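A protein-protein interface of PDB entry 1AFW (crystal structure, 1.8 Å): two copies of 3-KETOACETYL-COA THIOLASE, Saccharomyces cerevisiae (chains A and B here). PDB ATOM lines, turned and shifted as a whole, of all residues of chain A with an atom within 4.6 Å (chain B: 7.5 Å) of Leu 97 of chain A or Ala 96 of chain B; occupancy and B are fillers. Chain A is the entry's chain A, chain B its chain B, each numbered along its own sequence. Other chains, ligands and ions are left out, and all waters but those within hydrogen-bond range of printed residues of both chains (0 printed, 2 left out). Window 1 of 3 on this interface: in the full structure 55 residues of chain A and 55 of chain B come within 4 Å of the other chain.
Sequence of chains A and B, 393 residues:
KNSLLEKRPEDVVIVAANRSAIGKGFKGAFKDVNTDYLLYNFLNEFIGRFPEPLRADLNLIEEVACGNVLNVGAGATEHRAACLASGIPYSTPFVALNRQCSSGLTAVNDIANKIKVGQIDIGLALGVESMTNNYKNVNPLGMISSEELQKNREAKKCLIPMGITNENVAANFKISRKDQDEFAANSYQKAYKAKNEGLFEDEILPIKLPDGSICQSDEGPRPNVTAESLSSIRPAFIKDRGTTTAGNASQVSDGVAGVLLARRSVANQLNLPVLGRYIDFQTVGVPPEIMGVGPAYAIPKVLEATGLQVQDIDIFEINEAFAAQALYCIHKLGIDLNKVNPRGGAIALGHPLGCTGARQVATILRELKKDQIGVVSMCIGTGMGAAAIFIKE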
ATOM      1  N   ALA A  65      11.223 -21.950   5.981  1.00  0.00           N
ATOM      2  CA  ALA A  65      11.199 -21.980   7.482  1.00  0.00           C
ATOM      3  C   ALA A  65      11.058 -20.458   7.835  1.00  0.00           C
ATOM      4  O   ALA A  65      11.861 -19.626   7.394  1.00  0.00           O
ATOM      5  CB  ALA A  65      12.474 -22.514   8.070  1.00  0.00           C
ATOM      6  N   CYS A  66      10.076 -20.077   8.644  1.00  0.00           N
ATOM      7  CA  CYS A  66       9.815 -18.658   8.963  1.00  0.00           C
ATOM      8  C   CYS A  66       9.753 -18.410  10.436  1.00  0.00           C
ATOM      9  O   CYS A  66       8.891 -18.952  11.149  1.00  0.00           O
ATOM     10  CB  CYS A  66       8.426 -18.382   8.441  1.00  0.00           C
ATOM     11  SG  CYS A  66       8.071 -16.591   8.571  1.00  0.00           S
ATOM     12  N   GLY A  67      10.687 -17.621  10.943  1.00  0.00           N
ATOM     13  CA  GLY A  67      10.735 -17.284  12.380  1.00  0.00           C
ATOM     14  C   GLY A  67       9.694 -16.258  12.769  1.00  0.00           C
ATOM     15  O   GLY A  67       9.485 -15.297  12.034  1.00  0.00           O
ATOM     16  N   ASN A  68       9.082 -16.430  13.936  1.00  0.00           N
ATOM     17  CA  ASN A  68       8.073 -15.453  14.411  1.00  0.00           C
ATOM     18  C   ASN A  68       7.887 -15.695  15.882  1.00  0.00           C
ATOM     19  O   ASN A  68       7.872 -16.853  16.309  1.00  0.00           O
ATOM     20  CB  ASN A  68       6.740 -15.657  13.679  1.00  0.00           C
ATOM     21  CG  ASN A  68       5.679 -14.719  14.211  1.00  0.00           C
ATOM     22  OD1 ASN A  68       4.815 -15.167  14.959  1.00  0.00           O
ATOM     23  ND2 ASN A  68       5.733 -13.412  13.860  1.00  0.00           N
ATOM     24  N   VAL A  95       7.275 -24.299   7.609  1.00  0.00           N
ATOM     25  CA  VAL A  95       7.378 -24.595   9.056  1.00  0.00           C
ATOM     26  C   VAL A  95       7.590 -23.289   9.766  1.00  0.00           C
ATOM     27  O   VAL A  95       8.362 -22.508   9.248  1.00  0.00           O
ATOM     28  CB  VAL A  95       8.461 -25.679   9.446  1.00  0.00           C
ATOM     29  CG1 VAL A  95       9.867 -25.370   8.908  1.00  0.00           C
ATOM     30  CG2 VAL A  95       8.489 -25.827  10.908  1.00  0.00           C
ATOM     31  N   ALA A  96       6.933 -23.028  10.900  1.00  0.00           N
ATOM     32  CA  ALA A  96       7.113 -21.774  11.628  1.00  0.00           C
ATOM     33  C   ALA A  96       8.001 -22.127  12.803  1.00  0.00           C
ATOM     34  O   ALA A  96       7.823 -23.233  13.336  1.00  0.00           O
ATOM     35  CB  ALA A  96       5.772 -21.302  12.210  1.00  0.00           C
ATOM     36  N   LEU A  97       8.920 -21.251  13.242  1.00  0.00           N
ATOM     37  CA  LEU A  97       9.841 -21.570  14.390  1.00  0.00           C
ATOM     38  C   LEU A  97       9.933 -20.370  15.263  1.00  0.00           C
ATOM     39  O   LEU A  97       9.947 -19.227  14.826  1.00  0.00           O
ATOM     40  CB  LEU A  97      11.326 -21.795  13.945  1.00  0.00           C
ATOM     41  CG  LEU A  97      11.563 -22.654  12.724  1.00  0.00           C
ATOM     42  CD1 LEU A  97      12.893 -22.434  12.133  1.00  0.00           C
ATOM     43  CD2 LEU A  97      11.504 -24.038  13.256  1.00  0.00           C
ATOM     44  N   ASN A  98      10.042 -20.590  16.559  1.00  0.00           N
ATOM     45  CA  ASN A  98      10.149 -19.460  17.471  1.00  0.00           C
ATOM     46  C   ASN A  98      11.270 -19.833  18.435  1.00  0.00           C
ATOM     47  O   ASN A  98      11.149 -20.765  19.258  1.00  0.00           O
ATOM     48  CB  ASN A  98       8.832 -19.278  18.324  1.00  0.00           C
ATOM     49  CG  ASN A  98       8.965 -18.240  19.345  1.00  0.00           C
ATOM     50  OD1 ASN A  98       9.992 -17.527  19.374  1.00  0.00           O
ATOM     51  ND2 ASN A  98       7.952 -18.084  20.177  1.00  0.00           N
ATOM     52  N   ARG A  99      12.386 -19.115  18.329  1.00  0.00           N
ATOM     53  CA  ARG A  99      13.475 -19.330  19.300  1.00  0.00           C
ATOM     54  C   ARG A  99      13.697 -17.838  19.755  1.00  0.00           C
ATOM     55  O   ARG A  99      14.810 -17.259  19.744  1.00  0.00           O
ATOM     56  CB  ARG A  99      14.756 -19.950  18.749  1.00  0.00           C
ATOM     57  CG  ARG A  99      15.595 -20.348  20.000  1.00  0.00           C
ATOM     58  CD  ARG A  99      17.071 -20.637  19.648  1.00  0.00           C
ATOM     59  NE  ARG A  99      17.299 -21.709  18.637  1.00  0.00           N
ATOM     60  CZ  ARG A  99      17.488 -23.005  18.927  1.00  0.00           C
ATOM     61  NH1 ARG A  99      17.434 -23.347  20.208  1.00  0.00           N
ATOM     62  NH2 ARG A  99      17.708 -23.956  17.978  1.00  0.00           N
ATOM     63  N   SER A 103      14.899 -16.133  16.299  1.00  0.00           N
ATOM     64  CA  SER A 103      14.106 -16.945  15.343  1.00  0.00           C
ATOM     65  C   SER A 103      14.489 -16.843  13.874  1.00  0.00           C
ATOM     66  O   SER A 103      14.502 -17.808  13.122  1.00  0.00           O
ATOM     67  CB  SER A 103      12.600 -16.681  15.500  1.00  0.00           C
ATOM     68  OG  SER A 103      12.166 -16.803  16.856  1.00  0.00           O
ATOM     69  N   THR A 106      17.676 -18.696  13.526  1.00  0.00           N
ATOM     70  CA  THR A 106      17.407 -20.132  13.763  1.00  0.00           C
ATOM     71  C   THR A 106      16.774 -20.710  12.464  1.00  0.00           C
ATOM     72  O   THR A 106      16.970 -21.823  12.113  1.00  0.00           O
ATOM     73  CB  THR A 106      16.465 -20.309  14.914  1.00  0.00           C
ATOM     74  OG1 THR A 106      17.187 -20.124  16.144  1.00  0.00           O
ATOM     75  CG2 THR A 106      15.750 -21.641  14.899  1.00  0.00           C
ATOM     76  N   ALA A 107      16.045 -19.910  11.724  1.00  0.00           N
ATOM     77  CA  ALA A 107      15.417 -20.374  10.457  1.00  0.00           C
ATOM     78  C   ALA A 107      16.506 -20.654   9.457  1.00  0.00           C
ATOM     79  O   ALA A 107      16.420 -21.621   8.694  1.00  0.00           O
ATOM     80  CB  ALA A 107      14.391 -19.261   9.873  1.00  0.00           C
ATOM     81  N   ASP A 110      18.045 -23.954  10.351  1.00  0.00           N
ATOM     82  CA  ASP A 110      17.144 -25.062   9.960  1.00  0.00           C
ATOM     83  C   ASP A 110      17.273 -25.439   8.471  1.00  0.00           C
ATOM     84  O   ASP A 110      17.465 -26.620   8.115  1.00  0.00           O
ATOM     85  CB  ASP A 110      15.711 -24.622  10.350  1.00  0.00           C
ATOM     86  CG  ASP A 110      14.641 -25.677  10.100  1.00  0.00           C
ATOM     87  OD1 ASP A 110      14.050 -25.662   8.985  1.00  0.00           O
ATOM     88  OD2 ASP A 110      14.341 -26.450  11.048  1.00  0.00           O
ATOM     89  N   GLU B  63      19.785 -29.758  23.171  1.00  0.00           N
ATOM     90  CA  GLU B  63      18.703 -29.063  22.507  1.00  0.00           C
ATOM     91  C   GLU B  63      17.368 -29.731  22.877  1.00  0.00           C
ATOM     92  O   GLU B  63      17.268 -30.959  23.017  1.00  0.00           O
ATOM     93  CB  GLU B  63      18.879 -29.110  20.984  1.00  0.00           C
ATOM     94  CG  GLU B  63      17.754 -28.476  20.092  1.00  0.00           C
ATOM     95  CD  GLU B  63      17.913 -26.942  20.039  1.00  0.00           C
ATOM     96  OE1 GLU B  63      17.460 -26.247  20.969  1.00  0.00           O
ATOM     97  OE2 GLU B  63      18.470 -26.419  19.056  1.00  0.00           O
ATOM     98  N   VAL B  64      16.325 -28.904  22.952  1.00  0.00           N
ATOM     99  CA  VAL B  64      14.965 -29.396  23.182  1.00  0.00           C
ATOM    100  C   VAL B  64      14.171 -28.718  22.058  1.00  0.00           C
ATOM    101  O   VAL B  64      14.149 -27.452  21.989  1.00  0.00           O
ATOM    102  CB  VAL B  64      14.323 -28.931  24.544  1.00  0.00           C
ATOM    103  CG1 VAL B  64      12.907 -29.513  24.628  1.00  0.00           C
ATOM    104  CG2 VAL B  64      15.146 -29.523  25.721  1.00  0.00           C
ATOM    105  N   ALA B  65      13.531 -29.489  21.198  1.00  0.00           N
ATOM    106  CA  ALA B  65      12.732 -28.912  20.097  1.00  0.00           C
ATOM    107  C   ALA B  65      11.349 -29.350  20.450  1.00  0.00           C
ATOM    108  O   ALA B  65      11.109 -30.556  20.582  1.00  0.00           O
ATOM    109  CB  ALA B  65      13.134 -29.465  18.686  1.00  0.00           C
ATOM    110  N   CYS B  66      10.440 -28.403  20.630  1.00  0.00           N
ATOM    111  CA  CYS B  66       9.089 -28.812  21.036  1.00  0.00           C
ATOM    112  C   CYS B  66       8.031 -28.336  20.074  1.00  0.00           C
ATOM    113  O   CYS B  66       7.877 -27.138  19.838  1.00  0.00           O
ATOM    114  CB  CYS B  66       8.876 -28.184  22.414  1.00  0.00           C
ATOM    115  SG  CYS B  66       7.271 -28.630  23.217  1.00  0.00           S
ATOM    116  N   GLY B  67       7.295 -29.292  19.513  1.00  0.00           N
ATOM    117  CA  GLY B  67       6.219 -28.971  18.593  1.00  0.00           C
ATOM    118  C   GLY B  67       4.921 -28.524  19.316  1.00  0.00           C
ATOM    119  O   GLY B  67       4.548 -29.111  20.346  1.00  0.00           O
ATOM    120  N   ASN B  68       4.235 -27.523  18.758  1.00  0.00           N
ATOM    121  CA  ASN B  68       2.963 -27.005  19.358  1.00  0.00           C
ATOM    122  C   ASN B  68       2.291 -26.155  18.285  1.00  0.00           C
ATOM    123  O   ASN B  68       2.972 -25.481  17.498  1.00  0.00           O
ATOM    124  CB  ASN B  68       3.265 -26.223  20.612  1.00  0.00           C
ATOM    125  CG  ASN B  68       2.017 -25.543  21.204  1.00  0.00           C
ATOM    126  OD1 ASN B  68       1.765 -24.359  20.906  1.00  0.00           O
ATOM    127  ND2 ASN B  68       1.237 -26.272  21.994  1.00  0.00           N
ATOM    128  N   VAL B  72       0.198 -19.108  22.046  1.00  0.00           N
ATOM    129  CA  VAL B  72       0.802 -17.924  21.435  1.00  0.00           C
ATOM    130  C   VAL B  72       2.294 -18.240  21.267  1.00  0.00           C
ATOM    131  O   VAL B  72       2.898 -18.838  22.158  1.00  0.00           O
ATOM    132  CB  VAL B  72       0.644 -16.633  22.345  1.00  0.00           C
ATOM    133  CG1 VAL B  72       1.673 -15.499  22.008  1.00  0.00           C
ATOM    134  CG2 VAL B  72      -0.776 -16.107  22.194  1.00  0.00           C
ATOM    135  N   GLY B  73       2.882 -17.848  20.143  1.00  0.00           N
ATOM    136  CA  GLY B  73       4.294 -18.105  19.881  1.00  0.00           C
ATOM    137  C   GLY B  73       4.683 -19.606  19.795  1.00  0.00           C
ATOM    138  O   GLY B  73       5.863 -19.956  19.878  1.00  0.00           O
ATOM    139  N   ALA B  74       3.682 -20.475  19.663  1.00  0.00           N
ATOM    140  CA  ALA B  74       3.861 -21.928  19.652  1.00  0.00           C
ATOM    141  C   ALA B  74       4.404 -22.368  21.045  1.00  0.00           C
ATOM    142  O   ALA B  74       5.089 -23.374  21.165  1.00  0.00           O
ATOM    143  CB  ALA B  74       4.708 -22.418  18.510  1.00  0.00           C
ATOM    144  N   GLY B  75       4.103 -21.594  22.087  1.00  0.00           N
ATOM    145  CA  GLY B  75       4.416 -21.850  23.490  1.00  0.00           C
ATOM    146  C   GLY B  75       5.850 -21.791  23.925  1.00  0.00           C
ATOM    147  O   GLY B  75       6.207 -22.350  24.961  1.00  0.00           O
ATOM    148  N   ALA B  76       6.691 -21.110  23.171  1.00  0.00           N
ATOM    149  CA  ALA B  76       8.110 -21.101  23.557  1.00  0.00           C
ATOM    150  C   ALA B  76       8.448 -20.672  24.959  1.00  0.00           C
ATOM    151  O   ALA B  76       9.216 -21.308  25.626  1.00  0.00           O
ATOM    152  CB  ALA B  76       8.991 -20.282  22.555  1.00  0.00           C
ATOM    153  N   THR B  77       7.901 -19.556  25.380  1.00  0.00           N
ATOM    154  CA  THR B  77       8.189 -19.054  26.713  1.00  0.00           C
ATOM    155  C   THR B  77       7.849 -20.030  27.833  1.00  0.00           C
ATOM    156  O   THR B  77       8.708 -20.417  28.652  1.00  0.00           O
ATOM    157  CB  THR B  77       7.306 -17.801  26.934  1.00  0.00           C
ATOM    158  OG1 THR B  77       7.731 -16.821  25.994  1.00  0.00           O
ATOM    159  CG2 THR B  77       7.508 -17.286  28.354  1.00  0.00           C
ATOM    160  N   HIS B  79       6.983 -23.294  27.603  1.00  0.00           N
ATOM    161  CA  HIS B  79       7.531 -24.623  27.555  1.00  0.00           C
ATOM    162  C   HIS B  79       9.005 -24.649  27.969  1.00  0.00           C
ATOM    163  O   HIS B  79       9.465 -25.607  28.584  1.00  0.00           O
ATOM    164  CB  HIS B  79       7.321 -25.202  26.182  1.00  0.00           C
ATOM    165  CG  HIS B  79       5.879 -25.350  25.869  1.00  0.00           C
ATOM    166  ND1 HIS B  79       5.421 -25.535  24.580  1.00  0.00           N
ATOM    167  CD2 HIS B  79       4.791 -25.375  26.682  1.00  0.00           C
ATOM    168  CE1 HIS B  79       4.091 -25.589  24.618  1.00  0.00           C
ATOM    169  NE2 HIS B  79       3.685 -25.530  25.876  1.00  0.00           N
ATOM    170  N   PHE B  94      16.382 -24.143  23.778  1.00  0.00           N
ATOM    171  CA  PHE B  94      15.045 -24.618  23.511  1.00  0.00           C
ATOM    172  C   PHE B  94      14.478 -23.910  22.277  1.00  0.00           C
ATOM    173  O   PHE B  94      14.758 -22.739  22.191  1.00  0.00           O
ATOM    174  CB  PHE B  94      14.184 -24.155  24.681  1.00  0.00           C
ATOM    175  CG  PHE B  94      12.750 -24.531  24.523  1.00  0.00           C
ATOM    176  CD1 PHE B  94      11.877 -23.747  23.749  1.00  0.00           C
ATOM    177  CD2 PHE B  94      12.265 -25.682  25.111  1.00  0.00           C
ATOM    178  CE1 PHE B  94      10.568 -24.080  23.493  1.00  0.00           C
ATOM    179  CE2 PHE B  94      10.906 -26.029  24.928  1.00  0.00           C
ATOM    180  CZ  PHE B  94      10.060 -25.221  24.103  1.00  0.00           C
ATOM    181  N   VAL B  95      13.731 -24.591  21.386  1.00  0.00           N
ATOM    182  CA  VAL B  95      13.118 -23.989  20.211  1.00  0.00           C
ATOM    183  C   VAL B  95      11.713 -24.538  20.026  1.00  0.00           C
ATOM    184  O   VAL B  95      11.525 -25.732  20.176  1.00  0.00           O
ATOM    185  CB  VAL B  95      13.921 -24.223  18.959  1.00  0.00           C
ATOM    186  CG1 VAL B  95      14.136 -25.717  18.685  1.00  0.00           C
ATOM    187  CG2 VAL B  95      13.274 -23.494  17.808  1.00  0.00           C
ATOM    188  N   ALA B  96      10.717 -23.694  19.720  1.00  0.00           N
ATOM    189  CA  ALA B  96       9.341 -24.147  19.511  1.00  0.00           C
ATOM    190  C   ALA B  96       9.141 -24.241  17.984  1.00  0.00           C
ATOM    191  O   ALA B  96       9.627 -23.386  17.197  1.00  0.00           O
ATOM    192  CB  ALA B  96       8.387 -23.106  20.107  1.00  0.00           C
ATOM    193  N   LEU B  97       8.432 -25.272  17.541  1.00  0.00           N
ATOM    194  CA  LEU B  97       8.188 -25.438  16.103  1.00  0.00           C
ATOM    195  C   LEU B  97       6.699 -25.667  15.854  1.00  0.00           C
ATOM    196  O   LEU B  97       6.039 -26.367  16.638  1.00  0.00           O
ATOM    197  CB  LEU B  97       8.867 -26.751  15.633  1.00  0.00           C
ATOM    198  CG  LEU B  97      10.389 -26.655  15.789  1.00  0.00           C
ATOM    199  CD1 LEU B  97      10.782 -27.736  16.727  1.00  0.00           C
ATOM    200  CD2 LEU B  97      11.179 -26.756  14.481  1.00  0.00           C
ATOM    201  N   ASN B  98       6.194 -25.139  14.729  1.00  0.00           N
ATOM    202  CA  ASN B  98       4.805 -25.367  14.405  1.00  0.00           C
ATOM    203  C   ASN B  98       4.742 -25.748  12.942  1.00  0.00           C
ATOM    204  O   ASN B  98       4.946 -24.868  12.080  1.00  0.00           O
ATOM    205  CB  ASN B  98       3.957 -24.104  14.677  1.00  0.00           C
ATOM    206  CG  ASN B  98       2.460 -24.323  14.317  1.00  0.00           C
ATOM    207  OD1 ASN B  98       2.107 -25.441  13.951  1.00  0.00           O
ATOM    208  ND2 ASN B  98       1.617 -23.304  14.402  1.00  0.00           N
ATOM    209  N   ARG B  99       4.532 -27.042  12.665  1.00  0.00           N
ATOM    210  CA  ARG B  99       4.353 -27.516  11.311  1.00  0.00           C
ATOM    211  C   ARG B  99       2.934 -28.188  11.392  1.00  0.00           C
ATOM    212  O   ARG B  99       2.730 -29.337  10.991  1.00  0.00           O
ATOM    213  CB  ARG B  99       5.413 -28.483  10.775  1.00  0.00           C
ATOM    214  CG  ARG B  99       5.102 -28.634   9.267  1.00  0.00           C
ATOM    215  CD  ARG B  99       5.897 -29.635   8.429  1.00  0.00           C
ATOM    216  NE  ARG B  99       7.362 -29.600   8.539  1.00  0.00           N
ATOM    217  CZ  ARG B  99       8.178 -29.003   7.664  1.00  0.00           C
ATOM    218  NH1 ARG B  99       7.742 -28.306   6.606  1.00  0.00           N
ATOM    219  NH2 ARG B  99       9.475 -29.098   7.908  1.00  0.00           N
ATOM    220  N   THR B 106       8.063 -33.240  13.347  1.00  0.00           N
ATOM    221  CA  THR B 106       8.966 -32.289  12.758  1.00  0.00           C
ATOM    222  C   THR B 106      10.026 -32.031  13.804  1.00  0.00           C
ATOM    223  O   THR B 106      11.197 -31.783  13.496  1.00  0.00           O
ATOM    224  CB  THR B 106       8.154 -30.991  12.381  1.00  0.00           C
ATOM    225  OG1 THR B 106       7.666 -31.170  11.053  1.00  0.00           O
ATOM    226  CG2 THR B 106       8.965 -29.728  12.408  1.00  0.00           C
ATOM    227  N   ASP B 110      14.091 -32.297  13.362  1.00  0.00           N
ATOM    228  CA  ASP B 110      14.975 -31.196  13.738  1.00  0.00           C
ATOM    229  C   ASP B 110      16.154 -31.666  14.591  1.00  0.00           C
ATOM    230  O   ASP B 110      17.321 -31.261  14.416  1.00  0.00           O
ATOM    231  CB  ASP B 110      14.199 -30.160  14.571  1.00  0.00           C
ATOM    232  CG  ASP B 110      15.076 -28.930  14.943  1.00  0.00           C
ATOM    233  OD1 ASP B 110      15.303 -28.106  14.023  1.00  0.00           O
ATOM    234  OD2 ASP B 110      15.534 -28.769  16.122  1.00  0.00           O
ATOM    235  N   LYS B 114      20.220 -32.050  13.532  1.00  0.00           N
ATOM    236  CA  LYS B 114      21.276 -31.435  14.319  1.00  0.00           C
ATOM    237  C   LYS B 114      22.308 -32.460  14.718  1.00  0.00           C
ATOM    238  O   LYS B 114      23.504 -32.189  14.763  1.00  0.00           O
ATOM    239  CB  LYS B 114      20.742 -30.743  15.598  1.00  0.00           C
ATOM    240  CG  LYS B 114      20.149 -29.357  15.129  1.00  0.00           C
ATOM    241  CD  LYS B 114      19.197 -28.707  16.100  1.00  0.00           C
ATOM    242  CE  LYS B 114      18.642 -27.330  15.518  1.00  0.00           C
ATOM    243  NZ  LYS B 114      17.511 -26.920  16.459  1.00  0.00           N
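The backbone carbonyl oxygen of Ala 96 of chain A lies within hydrogen-bond range of the backbone NH of Asn 98 of chain B (2.9 Å).
The backbone carbonyl oxygen of Gly 73 of chain B lies within hydrogen-bond range of the side-chain amide nitrogen of Asn 98 of chain A, 2.8 Å away.
N of Asn 98 of chain A lies within hydrogen-bond range of O of Ala 96 of chain B (2.9 Å).
The guanidinium group (NH2) of Arg 99 of chain A is in salt-bridge range of the side-chain carboxylate (OE2) of Glu 63 of chain B, 2.8 Å away.
O of Phe 94 of chain B sits close to NH1 of Arg 99 of chain A (3.4 Å).
NZ of Lys 114 of chain B sits close to NH2 of Arg 99 of chain A.
The backbone NH of Cys 66 of chain A lies within hydrogen-bond range of the backbone carbonyl oxygen of Val 95 of chain A, 3.0 Å away.
The backbone NH of Leu 97 of chain A sits at hydrogen-bond distance from the backbone carbonyl oxygen of Cys 66 of chain A (3.1 Å).
OD1 of Asn 98 of chain A lies close to OG of Ser 103 of chain A (3.4 Å).
OG of Ser 103 of chain A lies within hydrogen-bond range of N of Arg 99 of chain A.
The backbone NH (N) of Cys 66 of chain B is in hydrogen-bond range of the backbone carbonyl oxygen (O) of Val 95 of chain B (2.9 Å).
The backbone NH (N) of Leu 97 of chain B sits at hydrogen-bond distance from the backbone carbonyl oxygen (O) of Cys 66 of chain B, 3.0 Å away.
Among the printed residues, merely in contact across the chains: Leu 97 of chain A with Leu 97 of chain B (3.0 Å), Leu 97 of chain A with Ala 96 of chain B (3.4 Å), Asn 98 of chain A with Ala 76 of chain B (3.4 Å), Asp 110 of chain A with Asp 110 of chain B (3.5 Å), Ala 96 of chain A with Leu 97 of chain B (3.6 Å), Asn 98 of chain A with Val 95 of chain B (3.8 Å), Arg 99 of chain A with Val 95 of chain B (3.8 Å), Val 95 of chain A with Arg 99 of chain B (3.8 Å) and Val 95 of chain A with Asn 98 of chain B (3.9 Å).
Leu 97 of chain A touches just these residues of chain B: Ala 96 and Leu 97.
Of chain A, only Leu 97 and Asn 98 come within 4 Å of Ala 96 of chain B.
Printed residues of chain A within 4 Å of Asn 98 of chain B: Val 95 and Ala 96.
Printed residues of chain A within 4 Å of Glu 63 of chain B: Arg 99 (2.8 Å).
Printed residues of chain A within 4 Å of Leu 97 of chain B: Ala 96 (3.6 Å) and Leu 97 (3.0 Å).
The nearest residue of chain B that does not touch Leu 97 of chain A is Val 95 of chain B (4.6 Å).
The nearest residue of chain A that does not touch Ala 96 of chain B is Ala 96 of chain A (4.3 Å).
The nearest printed residue of chain A that does not touch Leu 97 of chain B is Val 95 of chain A (4.6 Å).
Hydrophobic or aromatic side chains of chain B within 4 Å of the printed part of chain A: Ala 76, Val 95, Ala 96 and Leu 97.
Of the 13 printed residues of chain A, 6 touch a printed residue of chain B.
Printed residues of chain A that touch a printed residue of chain B: Val 95, Ala 96, Leu 97, Asn 98, Arg 99 and Asp 110.
Hydrophobic or aromatic side chains of chain A within 4 Å of the printed part of chain B: Val 95, Ala 96 and Leu 97.
Among the printed residues, 15 pairs touch across the chains.
Val 95 of chain A touches Asn 98 of chain B, and with the chains exchanged Asn 98 of chain A touches Val 95 of chain B.
Val 95 of chain A touches Arg 99 of chain B, and with the chains exchanged Arg 99 of chain A touches Val 95 of chain B.
Ala 96 of chain A touches Leu 97 of chain B, and with the chains exchanged Leu 97 of chain A touches Ala 96 of chain B.
Asp 110 of chain A touches its own counterpart, Asp 110 of chain B.
Of the 15 pairs that touch across the chains among the printed residues, 10 have their exchanged pair printed and touching as well.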
